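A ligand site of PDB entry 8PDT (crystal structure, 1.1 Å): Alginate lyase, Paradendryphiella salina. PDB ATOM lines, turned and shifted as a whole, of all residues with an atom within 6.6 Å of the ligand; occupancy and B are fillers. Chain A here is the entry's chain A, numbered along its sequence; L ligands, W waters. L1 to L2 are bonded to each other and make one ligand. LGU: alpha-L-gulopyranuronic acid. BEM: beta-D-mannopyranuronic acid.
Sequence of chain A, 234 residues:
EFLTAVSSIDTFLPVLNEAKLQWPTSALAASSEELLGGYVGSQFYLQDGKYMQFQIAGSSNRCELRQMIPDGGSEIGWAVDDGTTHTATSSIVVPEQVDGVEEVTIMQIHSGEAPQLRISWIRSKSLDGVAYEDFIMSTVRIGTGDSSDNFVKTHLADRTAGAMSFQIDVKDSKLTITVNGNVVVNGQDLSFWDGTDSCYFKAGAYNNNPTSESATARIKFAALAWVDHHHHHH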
ATOM      1  N   LYS A  20      24.505 -32.239 -22.211  1.00  0.00           N
ATOM      2  CA  LYS A  20      23.495 -32.603 -23.185  1.00  0.00           C
ATOM      3  C   LYS A  20      23.265 -31.410 -24.117  1.00  0.00           C
ATOM      4  O   LYS A  20      23.551 -30.266 -23.766  1.00  0.00           O
ATOM      5  CB  LYS A  20      22.187 -33.004 -22.498  1.00  0.00           C
ATOM      6  CG  LYS A  20      21.509 -31.841 -21.743  1.00  0.00           C
ATOM      7  CD  LYS A  20      20.188 -32.234 -21.094  1.00  0.00           C
ATOM      8  CE  LYS A  20      19.634 -31.062 -20.296  1.00  0.00           C
ATOM      9  NZ  LYS A  20      18.212 -31.279 -19.819  1.00  0.00           N
ATOM     10  N   GLN A  22      20.554 -29.187 -26.138  1.00  0.00           N
ATOM     11  CA  GLN A  22      19.173 -28.738 -26.215  1.00  0.00           C
ATOM     12  C   GLN A  22      18.972 -27.995 -27.533  1.00  0.00           C
ATOM     13  O   GLN A  22      19.726 -27.055 -27.841  1.00  0.00           O
ATOM     14  CB  GLN A  22      18.858 -27.829 -25.039  1.00  0.00           C
ATOM     15  CG  GLN A  22      18.891 -28.523 -23.696  1.00  0.00           C
ATOM     16  CD  GLN A  22      18.819 -27.551 -22.564  1.00  0.00           C
ATOM     17  OE1 GLN A  22      19.574 -26.579 -22.529  1.00  0.00           O
ATOM     18  NE2 GLN A  22      17.915 -27.803 -21.634  1.00  0.00           N
ATOM     19  N   THR A  25      14.550 -25.993 -28.799  1.00  0.00           N
ATOM     20  CA  THR A  25      14.127 -25.367 -27.548  1.00  0.00           C
ATOM     21  C   THR A  25      14.971 -25.969 -26.434  1.00  0.00           C
ATOM     22  O   THR A  25      16.064 -26.476 -26.684  1.00  0.00           O
ATOM     23  CB  THR A  25      12.634 -25.593 -27.280  1.00  0.00           C
ATOM     24  OG1 THR A  25      12.389 -26.998 -27.135  1.00  0.00           O
ATOM     25  CG2 THR A  25      11.792 -25.044 -28.420  1.00  0.00           C
ATOM     26  N   SER A  26      14.463 -25.965 -25.204  1.00  0.00           N
ATOM     27  CA  SER A  26      15.203 -26.677 -24.170  1.00  0.00           C
ATOM     28  C   SER A  26      14.929 -28.169 -24.168  1.00  0.00           C
ATOM     29  O   SER A  26      15.517 -28.885 -23.355  1.00  0.00           O
ATOM     30  CB  SER A  26      14.917 -26.092 -22.802  1.00  0.00           C
ATOM     31  OG  SER A  26      15.411 -24.779 -22.730  1.00  0.00           O
ATOM     32  N   ALA A  27      14.080 -28.639 -25.069  1.00  0.00           N
ATOM     33  CA  ALA A  27      13.925 -30.070 -25.287  1.00  0.00           C
ATOM     34  C   ALA A  27      15.259 -30.719 -25.625  1.00  0.00           C
ATOM     35  O   ALA A  27      16.116 -30.138 -26.308  1.00  0.00           O
ATOM     36  CB  ALA A  27      12.930 -30.314 -26.407  1.00  0.00           C
ATOM     37  N   LEU A  28      15.428 -31.950 -25.145  1.00  0.00           N
ATOM     38  CA  LEU A  28      16.621 -32.723 -25.409  1.00  0.00           C
ATOM     39  C   LEU A  28      16.734 -32.995 -26.897  1.00  0.00           C
ATOM     40  O   LEU A  28      15.783 -33.485 -27.524  1.00  0.00           O
ATOM     41  CB  LEU A  28      16.554 -34.042 -24.642  1.00  0.00           C
ATOM     42  CG  LEU A  28      17.767 -34.974 -24.812  1.00  0.00           C
ATOM     43  CD1 LEU A  28      19.023 -34.321 -24.257  1.00  0.00           C
ATOM     44  CD2 LEU A  28      17.512 -36.312 -24.136  1.00  0.00           C
ATOM     45  N   SER A  60      13.868 -16.870 -28.820  1.00  0.00           N
ATOM     46  CA  SER A  60      14.019 -17.687 -27.626  1.00  0.00           C
ATOM     47  C   SER A  60      14.359 -19.139 -27.930  1.00  0.00           C
ATOM     48  O   SER A  60      14.431 -19.944 -27.008  1.00  0.00           O
ATOM     49  CB  SER A  60      12.816 -17.612 -26.673  1.00  0.00           C
ATOM     50  N   ARG A  62      17.082 -22.132 -29.151  1.00  0.00           N
ATOM     51  CA  ARG A  62      18.478 -22.339 -28.811  1.00  0.00           C
ATOM     52  C   ARG A  62      19.023 -23.569 -29.511  1.00  0.00           C
ATOM     53  O   ARG A  62      18.308 -24.494 -29.874  1.00  0.00           O
ATOM     54  CB  ARG A  62      18.674 -22.496 -27.314  1.00  0.00           C
ATOM     55  CG  ARG A  62      18.125 -23.798 -26.746  1.00  0.00           C
ATOM     56  CD  ARG A  62      17.991 -23.716 -25.243  1.00  0.00           C
ATOM     57  NE  ARG A  62      16.877 -22.846 -24.838  1.00  0.00           N
ATOM     58  CZ  ARG A  62      16.947 -21.910 -23.896  1.00  0.00           C
ATOM     59  NH1 ARG A  62      18.088 -21.543 -23.349  1.00  0.00           N
ATOM     60  NH2 ARG A  62      15.828 -21.317 -23.505  1.00  0.00           N
ATOM     61  N   GLU A  64      22.160 -25.401 -27.676  1.00  0.00           N
ATOM     62  CA  GLU A  64      22.949 -25.054 -26.495  1.00  0.00           C
ATOM     63  C   GLU A  64      23.329 -26.321 -25.739  1.00  0.00           C
ATOM     64  O   GLU A  64      22.518 -27.218 -25.590  1.00  0.00           O
ATOM     65  CB  GLU A  64      22.107 -24.135 -25.578  1.00  0.00           C
ATOM     66  CG  GLU A  64      22.866 -23.201 -24.717  1.00  0.00           C
ATOM     67  CD  GLU A  64      21.965 -22.232 -23.962  1.00  0.00           C
ATOM     68  OE1 GLU A  64      20.740 -22.463 -23.805  1.00  0.00           O
ATOM     69  OE2 GLU A  64      22.522 -21.212 -23.486  1.00  0.00           O
ATOM     70  N   ARG A  66      24.198 -28.004 -22.110  1.00  0.00           N
ATOM     71  CA  ARG A  66      23.721 -27.825 -20.742  1.00  0.00           C
ATOM     72  C   ARG A  66      24.522 -28.778 -19.861  1.00  0.00           C
ATOM     73  O   ARG A  66      24.542 -29.983 -20.112  1.00  0.00           O
ATOM     74  CB  ARG A  66      22.229 -28.166 -20.704  1.00  0.00           C
ATOM     75  CG  ARG A  66      21.473 -27.829 -19.399  1.00  0.00           C
ATOM     76  CD  ARG A  66      21.783 -28.736 -18.228  1.00  0.00           C
ATOM     77  NE  ARG A  66      20.694 -28.651 -17.266  1.00  0.00           N
ATOM     78  CZ  ARG A  66      20.855 -28.788 -15.957  1.00  0.00           C
ATOM     79  NH1 ARG A  66      22.036 -29.034 -15.413  1.00  0.00           N
ATOM     80  NH2 ARG A  66      19.793 -28.667 -15.163  1.00  0.00           N
ATOM     81  N   GLN A  67      25.188 -28.243 -18.835  1.00  0.00           N
ATOM     82  CA  GLN A  67      26.111 -29.024 -18.015  1.00  0.00           C
ATOM     83  C   GLN A  67      25.435 -30.203 -17.332  1.00  0.00           C
ATOM     84  O   GLN A  67      24.394 -30.058 -16.682  1.00  0.00           O
ATOM     85  CB  GLN A  67      26.764 -28.114 -16.986  1.00  0.00           C
ATOM     86  CG  GLN A  67      27.852 -28.774 -16.157  1.00  0.00           C
ATOM     87  CD  GLN A  67      28.385 -27.889 -15.035  1.00  0.00           C
ATOM     88  OE1 GLN A  67      27.829 -26.844 -14.712  1.00  0.00           O
ATOM     89  NE2 GLN A  67      29.466 -28.340 -14.417  1.00  0.00           N
ATOM     90  N   MET A  68      26.068 -31.365 -17.449  1.00  0.00           N
ATOM     91  CA  MET A  68      25.619 -32.609 -16.843  1.00  0.00           C
ATOM     92  C   MET A  68      26.705 -33.185 -15.958  1.00  0.00           C
ATOM     93  O   MET A  68      27.894 -32.873 -16.098  1.00  0.00           O
ATOM     94  CB  MET A  68      25.256 -33.642 -17.926  1.00  0.00           C
ATOM     95  CG  MET A  68      24.260 -33.130 -18.945  1.00  0.00           C
ATOM     96  SD  MET A  68      22.578 -32.977 -18.282  1.00  0.00           S
ATOM     97  CE  MET A  68      22.078 -34.699 -18.274  1.00  0.00           C
ATOM     98  N   GLU A  75      21.359 -34.282 -14.879  1.00  0.00           N
ATOM     99  CA  GLU A  75      21.539 -32.836 -14.800  1.00  0.00           C
ATOM    100  C   GLU A  75      22.230 -32.438 -13.501  1.00  0.00           C
ATOM    101  O   GLU A  75      21.828 -32.859 -12.410  1.00  0.00           O
ATOM    102  CB  GLU A  75      20.169 -32.155 -14.859  1.00  0.00           C
ATOM    103  CG  GLU A  75      19.569 -32.071 -16.267  1.00  0.00           C
ATOM    104  CD  GLU A  75      18.906 -33.364 -16.734  1.00  0.00           C
ATOM    105  OE1 GLU A  75      18.764 -34.308 -15.934  1.00  0.00           O
ATOM    106  OE2 GLU A  75      18.517 -33.407 -17.933  1.00  0.00           O
ATOM    107  N   GLN A 108      26.200 -19.191 -20.265  1.00  0.00           N
ATOM    108  CA  GLN A 108      25.317 -18.841 -19.153  1.00  0.00           C
ATOM    109  C   GLN A 108      25.760 -19.527 -17.866  1.00  0.00           C
ATOM    110  O   GLN A 108      26.372 -20.591 -17.868  1.00  0.00           O
ATOM    111  CB  GLN A 108      23.870 -19.301 -19.387  1.00  0.00           C
ATOM    112  CG  GLN A 108      23.237 -18.788 -20.664  1.00  0.00           C
ATOM    113  CD  GLN A 108      21.715 -18.881 -20.632  1.00  0.00           C
ATOM    114  OE1 GLN A 108      21.064 -18.301 -19.755  1.00  0.00           O
ATOM    115  NE2 GLN A 108      21.150 -19.618 -21.569  1.00  0.00           N
ATOM    116  N   HIS A 110      22.876 -20.645 -15.268  1.00  0.00           N
ATOM    117  CA  HIS A 110      21.425 -20.694 -15.177  1.00  0.00           C
ATOM    118  C   HIS A 110      21.029 -21.639 -14.059  1.00  0.00           C
ATOM    119  O   HIS A 110      21.775 -22.547 -13.683  1.00  0.00           O
ATOM    120  CB  HIS A 110      20.817 -21.180 -16.518  1.00  0.00           C
ATOM    121  CG  HIS A 110      19.440 -20.676 -16.800  1.00  0.00           C
ATOM    122  ND1 HIS A 110      18.318 -21.182 -16.160  1.00  0.00           N
ATOM    123  CD2 HIS A 110      18.995 -19.741 -17.656  1.00  0.00           C
ATOM    124  CE1 HIS A 110      17.251 -20.551 -16.618  1.00  0.00           C
ATOM    125  NE2 HIS A 110      17.625 -19.661 -17.520  1.00  0.00           N
ATOM    126  N   SER A 111      19.826 -21.454 -13.506  1.00  0.00           N
ATOM    127  CA  SER A 111      19.301 -22.306 -12.447  1.00  0.00           C
ATOM    128  C   SER A 111      17.963 -22.877 -12.905  1.00  0.00           C
ATOM    129  O   SER A 111      17.583 -22.767 -14.068  1.00  0.00           O
ATOM    130  CB  SER A 111      19.161 -21.506 -11.171  1.00  0.00           C
ATOM    131  OG  SER A 111      18.150 -20.524 -11.345  1.00  0.00           O
ATOM    132  N   GLY A 112      17.224 -23.458 -11.961  1.00  0.00           N
ATOM    133  CA  GLY A 112      15.927 -23.976 -12.322  1.00  0.00           C
ATOM    134  C   GLY A 112      14.936 -22.919 -12.783  1.00  0.00           C
ATOM    135  O   GLY A 112      13.974 -23.249 -13.470  1.00  0.00           O
ATOM    136  N   ALA A 114      16.048 -19.150 -13.449  1.00  0.00           N
ATOM    137  CA  ALA A 114      16.535 -17.840 -13.873  1.00  0.00           C
ATOM    138  C   ALA A 114      17.939 -17.949 -14.415  1.00  0.00           C
ATOM    139  O   ALA A 114      18.718 -18.835 -14.007  1.00  0.00           O
ATOM    140  CB  ALA A 114      16.526 -16.845 -12.710  1.00  0.00           C
ATOM    141  N   TYR A 200      23.896 -24.279 -13.029  1.00  0.00           N
ATOM    142  CA  TYR A 200      24.675 -25.047 -13.981  1.00  0.00           C
ATOM    143  C   TYR A 200      25.177 -24.096 -15.069  1.00  0.00           C
ATOM    144  O   TYR A 200      24.631 -23.023 -15.288  1.00  0.00           O
ATOM    145  CB  TYR A 200      23.848 -26.171 -14.604  1.00  0.00           C
ATOM    146  CG  TYR A 200      22.536 -25.706 -15.186  1.00  0.00           C
ATOM    147  CD1 TYR A 200      21.388 -25.653 -14.417  1.00  0.00           C
ATOM    148  CD2 TYR A 200      22.427 -25.306 -16.518  1.00  0.00           C
ATOM    149  CE1 TYR A 200      20.177 -25.215 -14.915  1.00  0.00           C
ATOM    150  CE2 TYR A 200      21.203 -24.860 -17.053  1.00  0.00           C
ATOM    151  CZ  TYR A 200      20.085 -24.819 -16.245  1.00  0.00           C
ATOM    152  OH  TYR A 200      18.864 -24.393 -16.734  1.00  0.00           O
ATOM    153  N   LYS A 202      25.953 -23.296 -19.164  1.00  0.00           N
ATOM    154  CA  LYS A 202      25.484 -23.525 -20.523  1.00  0.00           C
ATOM    155  C   LYS A 202      26.411 -22.808 -21.494  1.00  0.00           C
ATOM    156  O   LYS A 202      27.048 -21.813 -21.143  1.00  0.00           O
ATOM    157  CB  LYS A 202      24.065 -23.010 -20.774  1.00  0.00           C
ATOM    158  CG  LYS A 202      23.040 -23.305 -19.697  1.00  0.00           C
ATOM    159  CD  LYS A 202      21.638 -23.078 -20.228  1.00  0.00           C
ATOM    160  CE  LYS A 202      21.085 -24.267 -20.983  1.00  0.00           C
ATOM    161  NZ  LYS A 202      19.844 -23.929 -21.726  1.00  0.00           N
ATOM    162  N   TYR A 206      21.846 -19.096 -27.986  1.00  0.00           N
ATOM    163  CA  TYR A 206      20.491 -18.900 -27.504  1.00  0.00           C
ATOM    164  C   TYR A 206      20.040 -17.531 -28.017  1.00  0.00           C
ATOM    165  O   TYR A 206      20.660 -16.511 -27.673  1.00  0.00           O
ATOM    166  CB  TYR A 206      20.478 -19.049 -25.979  1.00  0.00           C
ATOM    167  CG  TYR A 206      19.250 -18.615 -25.248  1.00  0.00           C
ATOM    168  CD1 TYR A 206      17.960 -18.864 -25.733  1.00  0.00           C
ATOM    169  CD2 TYR A 206      19.384 -17.978 -24.016  1.00  0.00           C
ATOM    170  CE1 TYR A 206      16.839 -18.477 -24.997  1.00  0.00           C
ATOM    171  CE2 TYR A 206      18.273 -17.580 -23.288  1.00  0.00           C
ATOM    172  CZ  TYR A 206      17.016 -17.836 -23.771  1.00  0.00           C
ATOM    173  OH  TYR A 206      15.921 -17.440 -23.018  1.00  0.00           O
HETATM  174  C1  LGU L   1      14.488 -30.052 -19.914  1.00  0.00           C
HETATM  175  C2  LGU L   1      13.752 -28.758 -20.244  1.00  0.00           C
HETATM  176  O2  LGU L   1      12.435 -29.087 -20.718  1.00  0.00           O
HETATM  177  C3  LGU L   1      13.670 -27.839 -19.068  1.00  0.00           C
HETATM  178  O3  LGU L   1      12.830 -28.421 -18.023  1.00  0.00           O
HETATM  179  C4  LGU L   1      15.021 -27.555 -18.467  1.00  0.00           C
HETATM  180  O4  LGU L   1      15.840 -26.794 -19.365  1.00  0.00           O
HETATM  181  C5  LGU L   1      15.743 -28.870 -18.181  1.00  0.00           C
HETATM  182  O5  LGU L   1      15.836 -29.698 -19.383  1.00  0.00           O
HETATM  183  C6  LGU L   1      17.114 -28.595 -17.652  1.00  0.00           C
HETATM  184  O6B LGU L   1      18.113 -29.034 -18.276  1.00  0.00           O
HETATM  185  O6A LGU L   1      17.245 -27.922 -16.587  1.00  0.00           O
HETATM  186  C1  BEM L   2      15.734 -25.381 -19.141  1.00  0.00           C
HETATM  187  C2  BEM L   2      17.027 -24.689 -19.483  1.00  0.00           C
HETATM  188  O2  BEM L   2      17.353 -25.028 -20.853  1.00  0.00           O
HETATM  189  C3  BEM L   2      16.902 -23.215 -19.288  1.00  0.00           C
HETATM  190  O3  BEM L   2      18.148 -22.596 -19.715  1.00  0.00           O
HETATM  191  C4  BEM L   2      15.715 -22.642 -20.019  1.00  0.00           C
HETATM  192  O4  BEM L   2      15.498 -21.294 -19.607  1.00  0.00           O
HETATM  193  C5  BEM L   2      14.427 -23.441 -19.751  1.00  0.00           C
HETATM  194  O5  BEM L   2      14.627 -24.854 -19.966  1.00  0.00           O
HETATM  195  C6  BEM L   2      13.361 -23.004 -20.715  1.00  0.00           C
HETATM  196  O6B BEM L   2      13.329 -23.466 -21.883  1.00  0.00           O
HETATM  197  O6A BEM L   2      12.488 -22.157 -20.348  1.00  0.00           O
HETATM  198  O   HOH W   1      11.028 -26.831 -21.727  1.00  0.00           O
HETATM  199  O   HOH W   2      16.689 -25.403 -15.648  1.00  0.00           O
HETATM  200  O   HOH W   3      14.145 -21.292 -16.441  1.00  0.00           O
HETATM  201  O   HOH W   4      12.895 -21.261 -23.462  1.00  0.00           O
HETATM  202  O   HOH W   5      18.074 -19.942 -20.939  1.00  0.00           O
HETATM  203  O   HOH W   6      10.709 -30.128 -18.601  1.00  0.00           O
HETATM  204  O   HOH W   7      12.529 -20.134 -18.656  1.00  0.00           O
HETATM  205  O   HOH W   8      11.730 -31.342 -22.358  1.00  0.00           O
HETATM  206  O   HOH W   9      16.661 -31.214 -22.302  1.00  0.00           O
HETATM  207  O   HOH W  10      11.941 -24.940 -23.973  1.00  0.00           O
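Glu 75 touches the ligand. OH of Tyr 200 touches C2 of BEM L2 (3.3 Å). Of the 21 residues printed, 9 come within 4 Å of the ligand.
The side-chain hydroxyl of Ser 26 is in hydrogen-bond range of an oxygen (O6B) of BEM L2, 2.6 Å away. O6B of LGU L1 is in salt-bridge range of NZ of Lys 20 (2.7 Å). The guanidinium group of Arg 66 is in salt-bridge range of an oxygen (O6B) of LGU L1, at 2.8 Å. NZ of Lys 202 lies within hydrogen-bond range of O2 of BEM L2 (2.9 Å). O2 of BEM L2 sits at hydrogen-bond distance from NE2 of Gln 22. NE2 of His 110 lies within hydrogen-bond range of O4 of BEM L2. NH2 of Arg 62 is in salt-bridge range of O6B of BEM L2 (3.7 Å).
The side-chain amide nitrogen of Gln 22 lies within hydrogen-bond range of the backbone carbonyl oxygen of Ser 26, 3.1 Å away. The side-chain hydroxyl (OG) of Ser 26 sits at hydrogen-bond distance from the guanidinium group (NE) of Arg 62, at 3.2 Å. O of Lys 20 sits at hydrogen-bond distance from N of Arg 66 (2.9 Å). The side-chain amino group (NZ) of Lys 20 lies within salt-bridge range of the side-chain carboxylate (OE2) of Glu 75, 2.9 Å away. The side-chain amino group (NZ) of Lys 202 is in salt-bridge range of the side-chain carboxylate (OE1) of Glu 64 (2.7 Å). The backbone NH (N) of Gln 22 is in hydrogen-bond range of the backbone carbonyl oxygen (O) of Glu 64, 2.8 Å away. The backbone carbonyl oxygen (O) of Ala 114 lies within hydrogen-bond range of a ring nitrogen (ND1) of His 110. The guanidinium group (NH1) of Arg 62 lies within salt-bridge range of the side-chain carboxylate (OE1) of Glu 64 (2.8 Å).
Water W2 lies within hydrogen-bond range of OH of Tyr 200 (2.6 Å), O6A of LGU L1 (2.7 Å) and O of Ser 111 (3.2 Å). Water W4 lies within hydrogen-bond range of an oxygen (O6B) of BEM L2 (2.7 Å) and the guanidinium group (NH2) of Arg 62 (2.9 Å). Water W10 bridges an oxygen (O6B) of BEM L2 (2.9 Å) and the backbone NH (N) of Ser 26 (3.0 Å). Water W5 lies within hydrogen-bond range of NH1 of Arg 62, O3 of BEM L2, NE2 of Gln 108 and NE2 of His 110. Water W9 lies within hydrogen-bond range of O of Ser 26 (2.8 Å), NZ of Lys 20 (2.9 Å), N of Leu 28 (3.2 Å) and O5 of LGU L1 (3.4 Å).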
